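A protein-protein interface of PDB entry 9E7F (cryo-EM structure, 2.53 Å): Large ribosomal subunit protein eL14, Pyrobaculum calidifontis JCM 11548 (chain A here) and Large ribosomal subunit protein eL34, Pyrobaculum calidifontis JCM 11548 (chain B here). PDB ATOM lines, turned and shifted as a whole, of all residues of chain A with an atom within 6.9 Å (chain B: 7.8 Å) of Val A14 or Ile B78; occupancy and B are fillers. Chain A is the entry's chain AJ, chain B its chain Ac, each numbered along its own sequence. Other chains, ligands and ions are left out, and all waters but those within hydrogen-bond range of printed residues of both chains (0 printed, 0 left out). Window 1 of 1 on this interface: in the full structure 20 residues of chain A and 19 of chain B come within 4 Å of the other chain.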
ATOM      1  N   VAL A  12      26.567  28.270 -24.192  1.00  0.00           N
ATOM      2  CA  VAL A  12      25.938  27.319 -25.096  1.00  0.00           C
ATOM      3  C   VAL A  12      24.786  28.031 -25.787  1.00  0.00           C
ATOM      4  O   VAL A  12      23.856  28.507 -25.126  1.00  0.00           O
ATOM      5  CB  VAL A  12      25.447  26.068 -24.357  1.00  0.00           C
ATOM      6  CG1 VAL A  12      24.698  25.161 -25.307  1.00  0.00           C
ATOM      7  CG2 VAL A  12      26.611  25.337 -23.731  1.00  0.00           C
ATOM      8  N   LYS A  13      24.852  28.116 -27.112  1.00  0.00           N
ATOM      9  CA  LYS A  13      23.765  28.718 -27.868  1.00  0.00           C
ATOM     10  C   LYS A  13      22.561  27.787 -27.886  1.00  0.00           C
ATOM     11  O   LYS A  13      22.690  26.584 -28.126  1.00  0.00           O
ATOM     12  CB  LYS A  13      24.216  29.038 -29.291  1.00  0.00           C
ATOM     13  CG  LYS A  13      23.157  29.747 -30.090  1.00  0.00           C
ATOM     14  CD  LYS A  13      23.739  30.691 -31.110  1.00  0.00           C
ATOM     15  CE  LYS A  13      22.654  31.154 -32.062  1.00  0.00           C
ATOM     16  NZ  LYS A  13      22.890  32.528 -32.560  1.00  0.00           N
ATOM     17  N   VAL A  14      21.382  28.349 -27.631  1.00  0.00           N
ATOM     18  CA  VAL A  14      20.189  27.550 -27.423  1.00  0.00           C
ATOM     19  C   VAL A  14      19.196  27.643 -28.578  1.00  0.00           C
ATOM     20  O   VAL A  14      18.396  26.720 -28.760  1.00  0.00           O
ATOM     21  CB  VAL A  14      19.512  27.933 -26.094  1.00  0.00           C
ATOM     22  CG1 VAL A  14      20.490  27.776 -24.956  1.00  0.00           C
ATOM     23  CG2 VAL A  14      18.994  29.349 -26.159  1.00  0.00           C
ATOM     24  N   LEU A  15      19.217  28.715 -29.362  1.00  0.00           N
ATOM     25  CA  LEU A  15      18.278  28.885 -30.459  1.00  0.00           C
ATOM     26  C   LEU A  15      19.022  28.932 -31.786  1.00  0.00           C
ATOM     27  O   LEU A  15      20.250  29.004 -31.839  1.00  0.00           O
ATOM     28  CB  LEU A  15      17.438  30.155 -30.281  1.00  0.00           C
ATOM     29  CG  LEU A  15      16.388  30.114 -29.174  1.00  0.00           C
ATOM     30  CD1 LEU A  15      15.408  31.255 -29.330  1.00  0.00           C
ATOM     31  CD2 LEU A  15      15.662  28.791 -29.189  1.00  0.00           C
ATOM     32  N   GLY A  16      18.254  28.889 -32.863  1.00  0.00           N
ATOM     33  CA  GLY A  16      18.812  28.977 -34.188  1.00  0.00           C
ATOM     34  C   GLY A  16      19.410  27.668 -34.663  1.00  0.00           C
ATOM     35  O   GLY A  16      19.275  26.613 -34.044  1.00  0.00           O
ATOM     36  N   GLU A  18      22.589  27.005 -34.835  1.00  0.00           N
ATOM     37  CA  GLU A  18      23.726  26.661 -33.998  1.00  0.00           C
ATOM     38  C   GLU A  18      23.330  26.345 -32.563  1.00  0.00           C
ATOM     39  O   GLU A  18      24.157  26.489 -31.658  1.00  0.00           O
ATOM     40  CB  GLU A  18      24.742  27.798 -34.013  1.00  0.00           C
ATOM     41  CG  GLU A  18      24.996  28.377 -35.379  1.00  0.00           C
ATOM     42  CD  GLU A  18      25.861  29.611 -35.321  1.00  0.00           C
ATOM     43  OE1 GLU A  18      26.264  30.109 -36.391  1.00  0.00           O
ATOM     44  OE2 GLU A  18      26.128  30.096 -34.205  1.00  0.00           O
ATOM     45  N   ALA A  19      22.090  25.933 -32.333  1.00  0.00           N
ATOM     46  CA  ALA A  19      21.650  25.624 -30.983  1.00  0.00           C
ATOM     47  C   ALA A  19      22.354  24.382 -30.460  1.00  0.00           C
ATOM     48  O   ALA A  19      22.616  23.436 -31.205  1.00  0.00           O
ATOM     49  CB  ALA A  19      20.137  25.424 -30.950  1.00  0.00           C
ATOM     50  N   GLY A  20      22.667  24.393 -29.167  1.00  0.00           N
ATOM     51  CA  GLY A  20      23.346  23.288 -28.531  1.00  0.00           C
ATOM     52  C   GLY A  20      24.850  23.314 -28.646  1.00  0.00           C
ATOM     53  O   GLY A  20      25.523  22.567 -27.926  1.00  0.00           O
ATOM     54  N   ARG A  21      25.402  24.157 -29.506  1.00  0.00           N
ATOM     55  CA  ARG A  21      26.837  24.258 -29.700  1.00  0.00           C
ATOM     56  C   ARG A  21      27.449  25.178 -28.652  1.00  0.00           C
ATOM     57  O   ARG A  21      26.754  25.928 -27.964  1.00  0.00           O
ATOM     58  CB  ARG A  21      27.143  24.768 -31.105  1.00  0.00           C
ATOM     59  CG  ARG A  21      27.286  23.656 -32.118  1.00  0.00           C
ATOM     60  CD  ARG A  21      27.820  24.168 -33.432  1.00  0.00           C
ATOM     61  NE  ARG A  21      26.954  23.820 -34.549  1.00  0.00           N
ATOM     62  CZ  ARG A  21      26.931  22.629 -35.131  1.00  0.00           C
ATOM     63  NH1 ARG A  21      27.700  21.640 -34.710  1.00  0.00           N
ATOM     64  NH2 ARG A  21      26.115  22.427 -36.159  1.00  0.00           N
ATOM     65  N   ASN A  53      19.700  36.438 -24.558  1.00  0.00           N
ATOM     66  CA  ASN A  53      18.646  35.490 -24.226  1.00  0.00           C
ATOM     67  C   ASN A  53      18.744  34.193 -25.015  1.00  0.00           C
ATOM     68  O   ASN A  53      18.082  33.217 -24.651  1.00  0.00           O
ATOM     69  CB  ASN A  53      17.279  36.123 -24.467  1.00  0.00           C
ATOM     70  CG  ASN A  53      16.950  37.189 -23.458  1.00  0.00           C
ATOM     71  OD1 ASN A  53      17.737  37.469 -22.559  1.00  0.00           O
ATOM     72  ND2 ASN A  53      15.794  37.809 -23.612  1.00  0.00           N
ATOM     73  N   HIS A  54      19.545  34.154 -26.076  1.00  0.00           N
ATOM     74  CA  HIS A  54      19.672  32.977 -26.919  1.00  0.00           C
ATOM     75  C   HIS A  54      20.900  32.152 -26.582  1.00  0.00           C
ATOM     76  O   HIS A  54      21.255  31.246 -27.341  1.00  0.00           O
ATOM     77  CB  HIS A  54      19.703  33.385 -28.388  1.00  0.00           C
ATOM     78  CG  HIS A  54      18.487  34.136 -28.826  1.00  0.00           C
ATOM     79  ND1 HIS A  54      18.481  34.972 -29.920  1.00  0.00           N
ATOM     80  CD2 HIS A  54      17.235  34.177 -28.315  1.00  0.00           C
ATOM     81  CE1 HIS A  54      17.279  35.498 -30.062  1.00  0.00           C
ATOM     82  NE2 HIS A  54      16.503  35.031 -29.101  1.00  0.00           N
ATOM     83  N   ILE A  55      21.559  32.448 -25.469  1.00  0.00           N
ATOM     84  CA  ILE A  55      22.723  31.702 -25.021  1.00  0.00           C
ATOM     85  C   ILE A  55      22.497  31.300 -23.577  1.00  0.00           C
ATOM     86  O   ILE A  55      21.768  31.966 -22.837  1.00  0.00           O
ATOM     87  CB  ILE A  55      24.021  32.520 -25.148  1.00  0.00           C
ATOM     88  CG1 ILE A  55      23.919  33.790 -24.307  1.00  0.00           C
ATOM     89  CG2 ILE A  55      24.299  32.848 -26.598  1.00  0.00           C
ATOM     90  CD1 ILE A  55      25.246  34.370 -23.923  1.00  0.00           C
ATOM     91  N   GLU A  56      23.122  30.200 -23.178  1.00  0.00           N
ATOM     92  CA  GLU A  56      23.094  29.767 -21.792  1.00  0.00           C
ATOM     93  C   GLU A  56      24.513  29.795 -21.250  1.00  0.00           C
ATOM     94  O   GLU A  56      25.380  29.074 -21.773  1.00  0.00           O
ATOM     95  CB  GLU A  56      22.498  28.370 -21.647  1.00  0.00           C
ATOM     96  CG  GLU A  56      22.453  27.881 -20.209  1.00  0.00           C
ATOM     97  CD  GLU A  56      21.293  28.466 -19.426  1.00  0.00           C
ATOM     98  OE1 GLU A  56      20.674  29.436 -19.910  1.00  0.00           O
ATOM     99  OE2 GLU A  56      21.000  27.959 -18.327  1.00  0.00           O
ATOM    100  N   VAL A  90      25.641  19.782 -26.697  1.00  0.00           N
ATOM    101  CA  VAL A  90      24.763  19.448 -25.586  1.00  0.00           C
ATOM    102  C   VAL A  90      23.579  18.629 -26.079  1.00  0.00           C
ATOM    103  O   VAL A  90      22.958  18.949 -27.100  1.00  0.00           O
ATOM    104  CB  VAL A  90      24.312  20.732 -24.877  1.00  0.00           C
ATOM    105  CG1 VAL A  90      23.593  20.399 -23.583  1.00  0.00           C
ATOM    106  CG2 VAL A  90      25.517  21.611 -24.610  1.00  0.00           C
ATOM    107  N   LYS A  91      23.263  17.559 -25.349  1.00  0.00           N
ATOM    108  CA  LYS A  91      22.215  16.634 -25.745  1.00  0.00           C
ATOM    109  C   LYS A  91      21.000  16.824 -24.853  1.00  0.00           C
ATOM    110  O   LYS A  91      21.058  16.477 -23.664  1.00  0.00           O
ATOM    111  CB  LYS A  91      22.715  15.193 -25.657  1.00  0.00           C
ATOM    112  CG  LYS A  91      23.607  14.766 -26.808  1.00  0.00           C
ATOM    113  CD  LYS A  91      22.891  14.885 -28.137  1.00  0.00           C
ATOM    114  CE  LYS A  91      21.481  14.334 -28.063  1.00  0.00           C
ATOM    115  NZ  LYS A  91      20.540  15.172 -28.850  1.00  0.00           N
ATOM    116  N   PRO A  92      19.893  17.352 -25.361  1.00  0.00           N
ATOM    117  CA  PRO A  92      18.713  17.553 -24.522  1.00  0.00           C
ATOM    118  C   PRO A  92      17.959  16.254 -24.288  1.00  0.00           C
ATOM    119  O   PRO A  92      18.057  15.295 -25.052  1.00  0.00           O
ATOM    120  CB  PRO A  92      17.870  18.532 -25.340  1.00  0.00           C
ATOM    121  CG  PRO A  92      18.218  18.217 -26.744  1.00  0.00           C
ATOM    122  CD  PRO A  92      19.648  17.745 -26.759  1.00  0.00           C
ATOM    123  N   LYS A  93      17.189  16.246 -23.204  1.00  0.00           N
ATOM    124  CA  LYS A  93      16.301  15.137 -22.865  1.00  0.00           C
ATOM    125  C   LYS A  93      14.872  15.655 -22.974  1.00  0.00           C
ATOM    126  O   LYS A  93      14.301  16.149 -22.003  1.00  0.00           O
ATOM    127  CB  LYS A  93      16.591  14.599 -21.473  1.00  0.00           C
ATOM    128  CG  LYS A  93      18.041  14.244 -21.243  1.00  0.00           C
ATOM    129  CD  LYS A  93      18.576  14.944 -20.007  1.00  0.00           C
ATOM    130  CE  LYS A  93      18.846  16.416 -20.279  1.00  0.00           C
ATOM    131  NZ  LYS A  93      19.316  17.125 -19.062  1.00  0.00           N
ATOM    132  N   LEU A  94      14.293  15.531 -24.168  1.00  0.00           N
ATOM    133  CA  LEU A  94      12.971  16.096 -24.409  1.00  0.00           C
ATOM    134  C   LEU A  94      11.881  15.352 -23.648  1.00  0.00           C
ATOM    135  O   LEU A  94      10.808  15.914 -23.397  1.00  0.00           O
ATOM    136  CB  LEU A  94      12.676  16.097 -25.905  1.00  0.00           C
ATOM    137  CG  LEU A  94      13.879  16.442 -26.780  1.00  0.00           C
ATOM    138  CD1 LEU A  94      13.523  16.324 -28.248  1.00  0.00           C
ATOM    139  CD2 LEU A  94      14.373  17.837 -26.465  1.00  0.00           C
ATOM    140  N   ILE A  97      10.607  17.035 -20.453  1.00  0.00           N
ATOM    141  CA  ILE A  97       9.925  18.318 -20.564  1.00  0.00           C
ATOM    142  C   ILE A  97       8.421  18.098 -20.615  1.00  0.00           C
ATOM    143  O   ILE A  97       7.932  17.152 -21.241  1.00  0.00           O
ATOM    144  CB  ILE A  97      10.429  19.085 -21.798  1.00  0.00           C
ATOM    145  CG1 ILE A  97      11.932  19.311 -21.688  1.00  0.00           C
ATOM    146  CG2 ILE A  97       9.719  20.413 -21.932  1.00  0.00           C
ATOM    147  CD1 ILE A  97      12.296  20.531 -20.890  1.00  0.00           C
ATOM    148  N   ARG B  63      17.342  23.593 -37.582  1.00  0.00           N
ATOM    149  CA  ARG B  63      17.634  23.546 -36.162  1.00  0.00           C
ATOM    150  C   ARG B  63      17.869  22.097 -35.780  1.00  0.00           C
ATOM    151  O   ARG B  63      17.426  21.194 -36.498  1.00  0.00           O
ATOM    152  CB  ARG B  63      16.488  24.137 -35.328  1.00  0.00           C
ATOM    153  CG  ARG B  63      16.927  24.703 -33.998  1.00  0.00           C
ATOM    154  CD  ARG B  63      15.784  25.350 -33.238  1.00  0.00           C
ATOM    155  NE  ARG B  63      14.479  24.858 -33.655  1.00  0.00           N
ATOM    156  CZ  ARG B  63      13.538  25.616 -34.197  1.00  0.00           C
ATOM    157  NH1 ARG B  63      13.726  26.908 -34.402  1.00  0.00           N
ATOM    158  NH2 ARG B  63      12.380  25.065 -34.544  1.00  0.00           N
ATOM    159  N   PRO B  64      18.597  21.842 -34.694  1.00  0.00           N
ATOM    160  CA  PRO B  64      18.630  20.487 -34.141  1.00  0.00           C
ATOM    161  C   PRO B  64      17.232  20.025 -33.766  1.00  0.00           C
ATOM    162  O   PRO B  64      16.432  20.793 -33.234  1.00  0.00           O
ATOM    163  CB  PRO B  64      19.530  20.626 -32.911  1.00  0.00           C
ATOM    164  CG  PRO B  64      20.370  21.802 -33.186  1.00  0.00           C
ATOM    165  CD  PRO B  64      19.613  22.717 -34.093  1.00  0.00           C
ATOM    166  N   TYR B  65      16.937  18.770 -34.106  1.00  0.00           N
ATOM    167  CA  TYR B  65      15.671  18.086 -33.854  1.00  0.00           C
ATOM    168  C   TYR B  65      14.534  18.540 -34.768  1.00  0.00           C
ATOM    169  O   TYR B  65      13.449  17.954 -34.724  1.00  0.00           O
ATOM    170  CB  TYR B  65      15.267  18.220 -32.387  1.00  0.00           C
ATOM    171  CG  TYR B  65      16.059  17.309 -31.488  1.00  0.00           C
ATOM    172  CD1 TYR B  65      17.346  17.638 -31.094  1.00  0.00           C
ATOM    173  CD2 TYR B  65      15.529  16.107 -31.051  1.00  0.00           C
ATOM    174  CE1 TYR B  65      18.073  16.806 -30.287  1.00  0.00           C
ATOM    175  CE2 TYR B  65      16.251  15.267 -30.243  1.00  0.00           C
ATOM    176  CZ  TYR B  65      17.520  15.622 -29.863  1.00  0.00           C
ATOM    177  OH  TYR B  65      18.244  14.781 -29.054  1.00  0.00           O
ATOM    178  N   HIS B  71      10.792  25.458 -30.921  1.00  0.00           N
ATOM    179  CA  HIS B  71      11.996  26.107 -30.420  1.00  0.00           C
ATOM    180  C   HIS B  71      11.940  26.295 -28.912  1.00  0.00           C
ATOM    181  O   HIS B  71      12.984  26.326 -28.253  1.00  0.00           O
ATOM    182  CB  HIS B  71      12.208  27.443 -31.134  1.00  0.00           C
ATOM    183  CG  HIS B  71      11.288  28.530 -30.680  1.00  0.00           C
ATOM    184  ND1 HIS B  71       9.964  28.592 -31.057  1.00  0.00           N
ATOM    185  CD2 HIS B  71      11.502  29.604 -29.886  1.00  0.00           C
ATOM    186  CE1 HIS B  71       9.402  29.653 -30.510  1.00  0.00           C
ATOM    187  NE2 HIS B  71      10.315  30.285 -29.796  1.00  0.00           N
ATOM    188  N   LYS B  72      10.738  26.402 -28.345  1.00  0.00           N
ATOM    189  CA  LYS B  72      10.601  26.609 -26.906  1.00  0.00           C
ATOM    190  C   LYS B  72      11.039  25.378 -26.125  1.00  0.00           C
ATOM    191  O   LYS B  72      11.757  25.482 -25.126  1.00  0.00           O
ATOM    192  CB  LYS B  72       9.156  26.966 -26.569  1.00  0.00           C
ATOM    193  CG  LYS B  72       9.021  28.081 -25.573  1.00  0.00           C
ATOM    194  CD  LYS B  72       8.968  29.417 -26.270  1.00  0.00           C
ATOM    195  CE  LYS B  72       7.778  29.492 -27.194  1.00  0.00           C
ATOM    196  NZ  LYS B  72       6.505  29.275 -26.461  1.00  0.00           N
ATOM    197  N   VAL B  73      10.601  24.200 -26.562  1.00  0.00           N
ATOM    198  CA  VAL B  73      10.980  22.967 -25.888  1.00  0.00           C
ATOM    199  C   VAL B  73      12.461  22.684 -26.079  1.00  0.00           C
ATOM    200  O   VAL B  73      13.133  22.194 -25.166  1.00  0.00           O
ATOM    201  CB  VAL B  73      10.114  21.802 -26.393  1.00  0.00           C
ATOM    202  CG1 VAL B  73      10.621  20.491 -25.837  1.00  0.00           C
ATOM    203  CG2 VAL B  73       8.660  22.027 -26.019  1.00  0.00           C
ATOM    204  N   LEU B  74      12.991  22.977 -27.266  1.00  0.00           N
ATOM    205  CA  LEU B  74      14.387  22.665 -27.547  1.00  0.00           C
ATOM    206  C   LEU B  74      15.325  23.539 -26.729  1.00  0.00           C
ATOM    207  O   LEU B  74      16.290  23.045 -26.137  1.00  0.00           O
ATOM    208  CB  LEU B  74      14.676  22.832 -29.036  1.00  0.00           C
ATOM    209  CG  LEU B  74      16.136  22.613 -29.430  1.00  0.00           C
ATOM    210  CD1 LEU B  74      16.507  21.149 -29.332  1.00  0.00           C
ATOM    211  CD2 LEU B  74      16.398  23.135 -30.818  1.00  0.00           C
ATOM    212  N   ALA B  75      15.064  24.845 -26.699  1.00  0.00           N
ATOM    213  CA  ALA B  75      15.941  25.762 -25.981  1.00  0.00           C
ATOM    214  C   ALA B  75      15.920  25.484 -24.486  1.00  0.00           C
ATOM    215  O   ALA B  75      16.965  25.491 -23.827  1.00  0.00           O
ATOM    216  CB  ALA B  75      15.529  27.204 -26.263  1.00  0.00           C
ATOM    217  N   ARG B  76      14.732  25.229 -23.937  1.00  0.00           N
ATOM    218  CA  ARG B  76      14.613  24.961 -22.510  1.00  0.00           C
ATOM    219  C   ARG B  76      15.290  23.651 -22.138  1.00  0.00           C
ATOM    220  O   ARG B  76      15.937  23.552 -21.091  1.00  0.00           O
ATOM    221  CB  ARG B  76      13.139  24.950 -22.108  1.00  0.00           C
ATOM    222  CG  ARG B  76      12.816  24.062 -20.929  1.00  0.00           C
ATOM    223  CD  ARG B  76      13.287  24.665 -19.628  1.00  0.00           C
ATOM    224  NE  ARG B  76      13.293  26.120 -19.662  1.00  0.00           N
ATOM    225  CZ  ARG B  76      14.062  26.878 -18.893  1.00  0.00           C
ATOM    226  NH1 ARG B  76      14.896  26.349 -18.017  1.00  0.00           N
ATOM    227  NH2 ARG B  76      13.994  28.200 -19.010  1.00  0.00           N
ATOM    228  N   ALA B  77      15.148  22.631 -22.984  1.00  0.00           N
ATOM    229  CA  ALA B  77      15.783  21.349 -22.703  1.00  0.00           C
ATOM    230  C   ALA B  77      17.298  21.473 -22.721  1.00  0.00           C
ATOM    231  O   ALA B  77      17.986  20.857 -21.901  1.00  0.00           O
ATOM    232  CB  ALA B  77      15.318  20.296 -23.706  1.00  0.00           C
ATOM    233  N   ILE B  78      17.830  22.277 -23.642  1.00  0.00           N
ATOM    234  CA  ILE B  78      19.270  22.503 -23.711  1.00  0.00           C
ATOM    235  C   ILE B  78      19.763  23.209 -22.459  1.00  0.00           C
ATOM    236  O   ILE B  78      20.881  22.965 -21.993  1.00  0.00           O
ATOM    237  CB  ILE B  78      19.626  23.301 -24.977  1.00  0.00           C
ATOM    238  CG1 ILE B  78      19.332  22.478 -26.228  1.00  0.00           C
ATOM    239  CG2 ILE B  78      21.081  23.723 -24.945  1.00  0.00           C
ATOM    240  CD1 ILE B  78      19.460  23.267 -27.504  1.00  0.00           C
ATOM    241  N   ARG B  79      18.948  24.112 -21.907  1.00  0.00           N
ATOM    242  CA  ARG B  79      19.313  24.782 -20.664  1.00  0.00           C
ATOM    243  C   ARG B  79      19.430  23.789 -19.517  1.00  0.00           C
ATOM    244  O   ARG B  79      20.348  23.883 -18.696  1.00  0.00           O
ATOM    245  CB  ARG B  79      18.284  25.858 -20.329  1.00  0.00           C
ATOM    246  CG  ARG B  79      18.454  27.149 -21.099  1.00  0.00           C
ATOM    247  CD  ARG B  79      17.644  28.267 -20.471  1.00  0.00           C
ATOM    248  NE  ARG B  79      17.140  29.206 -21.464  1.00  0.00           N
ATOM    249  CZ  ARG B  79      17.847  30.198 -21.985  1.00  0.00           C
ATOM    250  NH1 ARG B  79      19.100  30.414 -21.626  1.00  0.00           N
ATOM    251  NH2 ARG B  79      17.282  30.993 -22.887  1.00  0.00           N
ATOM    252  N   TYR B  80      18.501  22.837 -19.439  1.00  0.00           N
ATOM    253  CA  TYR B  80      18.560  21.825 -18.391  1.00  0.00           C
ATOM    254  C   TYR B  80      19.779  20.932 -18.554  1.00  0.00           C
ATOM    255  O   TYR B  80      20.428  20.570 -17.568  1.00  0.00           O
ATOM    256  CB  TYR B  80      17.287  20.980 -18.403  1.00  0.00           C
ATOM    257  CG  TYR B  80      16.086  21.637 -17.773  1.00  0.00           C
ATOM    258  CD1 TYR B  80      16.197  22.847 -17.113  1.00  0.00           C
ATOM    259  CD2 TYR B  80      14.840  21.041 -17.839  1.00  0.00           C
ATOM    260  CE1 TYR B  80      15.098  23.442 -16.537  1.00  0.00           C
ATOM    261  CE2 TYR B  80      13.737  21.626 -17.267  1.00  0.00           C
ATOM    262  CZ  TYR B  80      13.869  22.826 -16.617  1.00  0.00           C
ATOM    263  OH  TYR B  80      12.762  23.407 -16.047  1.00  0.00           O
ATOM    264  N   ALA B  81      20.097  20.556 -19.791  1.00  0.00           N
ATOM    265  CA  ALA B  81      21.250  19.698 -20.027  1.00  0.00           C
ATOM    266  C   ALA B  81      22.549  20.410 -19.679  1.00  0.00           C
ATOM    267  O   ALA B  81      23.523  19.773 -19.265  1.00  0.00           O
ATOM    268  CB  ALA B  81      21.264  19.233 -21.482  1.00  0.00           C
ATOM    269  N   VAL B  82      22.582  21.733 -19.844  1.00  0.00           N
ATOM    270  CA  VAL B  82      23.786  22.495 -19.531  1.00  0.00           C
ATOM    271  C   VAL B  82      24.054  22.472 -18.031  1.00  0.00           C
ATOM    272  O   VAL B  82      25.194  22.301 -17.588  1.00  0.00           O
ATOM    273  CB  VAL B  82      23.660  23.933 -20.059  1.00  0.00           C
ATOM    274  CG1 VAL B  82      24.619  24.846 -19.332  1.00  0.00           C
ATOM    275  CG2 VAL B  82      23.912  23.965 -21.548  1.00  0.00           C
ATOM    276  N   ARG B  83      23.010  22.660 -17.229  1.00  0.00           N
ATOM    277  CA  ARG B  83      23.180  22.648 -15.783  1.00  0.00           C
ATOM    278  C   ARG B  83      23.305  21.240 -15.224  1.00  0.00           C
ATOM    279  O   ARG B  83      23.998  21.035 -14.222  1.00  0.00           O
ATOM    280  CB  ARG B  83      22.015  23.369 -15.115  1.00  0.00           C
ATOM    281  CG  ARG B  83      21.771  24.740 -15.681  1.00  0.00           C
ATOM    282  CD  ARG B  83      20.467  25.306 -15.203  1.00  0.00           C
ATOM    283  NE  ARG B  83      19.992  26.351 -16.096  1.00  0.00           N
ATOM    284  CZ  ARG B  83      18.731  26.739 -16.180  1.00  0.00           C
ATOM    285  NH1 ARG B  83      17.790  26.191 -15.431  1.00  0.00           N
ATOM    286  NH2 ARG B  83      18.405  27.701 -17.034  1.00  0.00           N
ATOM    287  N   ARG B  84      22.641  20.271 -15.840  1.00  0.00           N
ATOM    288  CA  ARG B  84      22.621  18.903 -15.344  1.00  0.00           C
ATOM    289  C   ARG B  84      23.948  18.210 -15.604  1.00  0.00           C
ATOM    290  O   ARG B  84      24.993  18.664 -15.140  1.00  0.00           O
ATOM    291  CB  ARG B  84      21.476  18.132 -15.994  1.00  0.00           C
ATOM    292  CG  ARG B  84      20.921  16.997 -15.165  1.00  0.00           C
ATOM    293  CD  ARG B  84      19.416  16.887 -15.341  1.00  0.00           C
ATOM    294  NE  ARG B  84      18.695  17.797 -14.457  1.00  0.00           N
ATOM    295  CZ  ARG B  84      18.361  19.046 -14.760  1.00  0.00           C
ATOM    296  NH1 ARG B  84      18.669  19.580 -15.928  1.00  0.00           N
ATOM    297  NH2 ARG B  84      17.700  19.777 -13.868  1.00  0.00           N
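Among the printed residues, pairs that only touch across the chains: Gly A16 with Arg B63, Leu A15 with Ala B75, Val A90 with Ala B81, Lys A93 with Ala B81, Ala A19 with Pro B64, Leu A94 with Tyr B65, Pro A92 with Ala B77, Lys A91 with Ala B81, Ile A97 with Arg B76, Lys A93 with Arg B84, Val A12 with Val B82, Leu A15 with His B71, Gly A20 with Ile B78, Leu A94 with Ala B77, Pro A92 with Tyr B65, Val A14 with Ile B78, Val A14 with Ala B75, Glu A56 with Val B82, Lys A93 with Tyr B80, Val A12 with Ile B78 and Gly A16 with Pro B64.
The backbone carbonyl oxygen (O) of Asn A53 lies within hydrogen-bond range of the guanidinium group (NH2) of Arg B79, 2.9 Å away. O of Ile A55 is in hydrogen-bond range of NH1 of Arg B79 (3.3 Å). The side-chain carboxylate (OE1) of Glu A56 is in salt-bridge range of the guanidinium group (NH1) of Arg B79, 2.5 Å away. The guanidinium group (NH2) of Arg B83 lies within salt-bridge range of the side-chain carboxylate (OE2) of Glu A56, 2.9 Å away. The side-chain amino group (NZ) of Lys A91 lies close to the side-chain hydroxyl (OH) of Tyr B65, 2.3 Å away.
The backbone carbonyl oxygen (O) of Val A12 lies within hydrogen-bond range of the backbone NH (N) of Glu A56 (2.7 Å). O of Lys A13 is in hydrogen-bond range of N of Gly A20 (2.4 Å). The backbone carbonyl oxygen (O) of His A54 sits at hydrogen-bond distance from the backbone NH (N) of Val A14, at 2.9 Å. The backbone carbonyl oxygen (O) of Gly A20 sits at hydrogen-bond distance from the backbone NH (N) of Val A90, at 3.0 Å. The backbone carbonyl oxygen (O) of Tyr B80 is in hydrogen-bond range of the guanidinium group (NH1) of Arg B84, 2.6 Å away.
Printed residues of chain B that touch a printed residue of chain A: Arg B63, Pro B64, Tyr B65, His B71, Ala B75, Arg B76, Ala B77, Ile B78, Arg B79, Tyr B80, Ala B81, Val B82, Arg B83 and Arg B84. Hydrophobic or aromatic side chains of chain B within 4 Å of the printed part of chain A: Pro B64, Tyr B65, Ala B75, Ala B77, Ile B78, Ala B81 and Val B82.
Of chain B, only Ala B75 (3.8 Å) and Ile B78 (3.8 Å) come within 4 Å of Val A14. Of the printed residues of chain B, Gly A16 touches Arg B63 (3.0 Å) and Pro B64 (3.9 Å). Arg A21 touches none of the printed residues of chain B. Of the printed residues of chain B, Val A90 touches Ala B81 (3.3 Å). Of the printed residues of chain A, His B71 touches Leu A15. Ile B78 touches just these residues of chain A: Val A12 (3.9 Å), Val A14 (3.8 Å) and Gly A20 (3.8 Å). Printed residues of chain A within 4 Å of Tyr B80: Lys A93. Printed residues of chain A within 4 Å of Ala B81: Val A90 (3.3 Å), Lys A91 (3.5 Å) and Lys A93 (3.4 Å). The nearest residue of chain B that does not touch Val A14 is Arg B79 (4.04 Å). The nearest residue of chain A that does not touch Ile B78 is Val A90 (4.1 Å). The nearest printed residue of chain B that does not touch Asn A53 is Ala B75 (6.7 Å).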
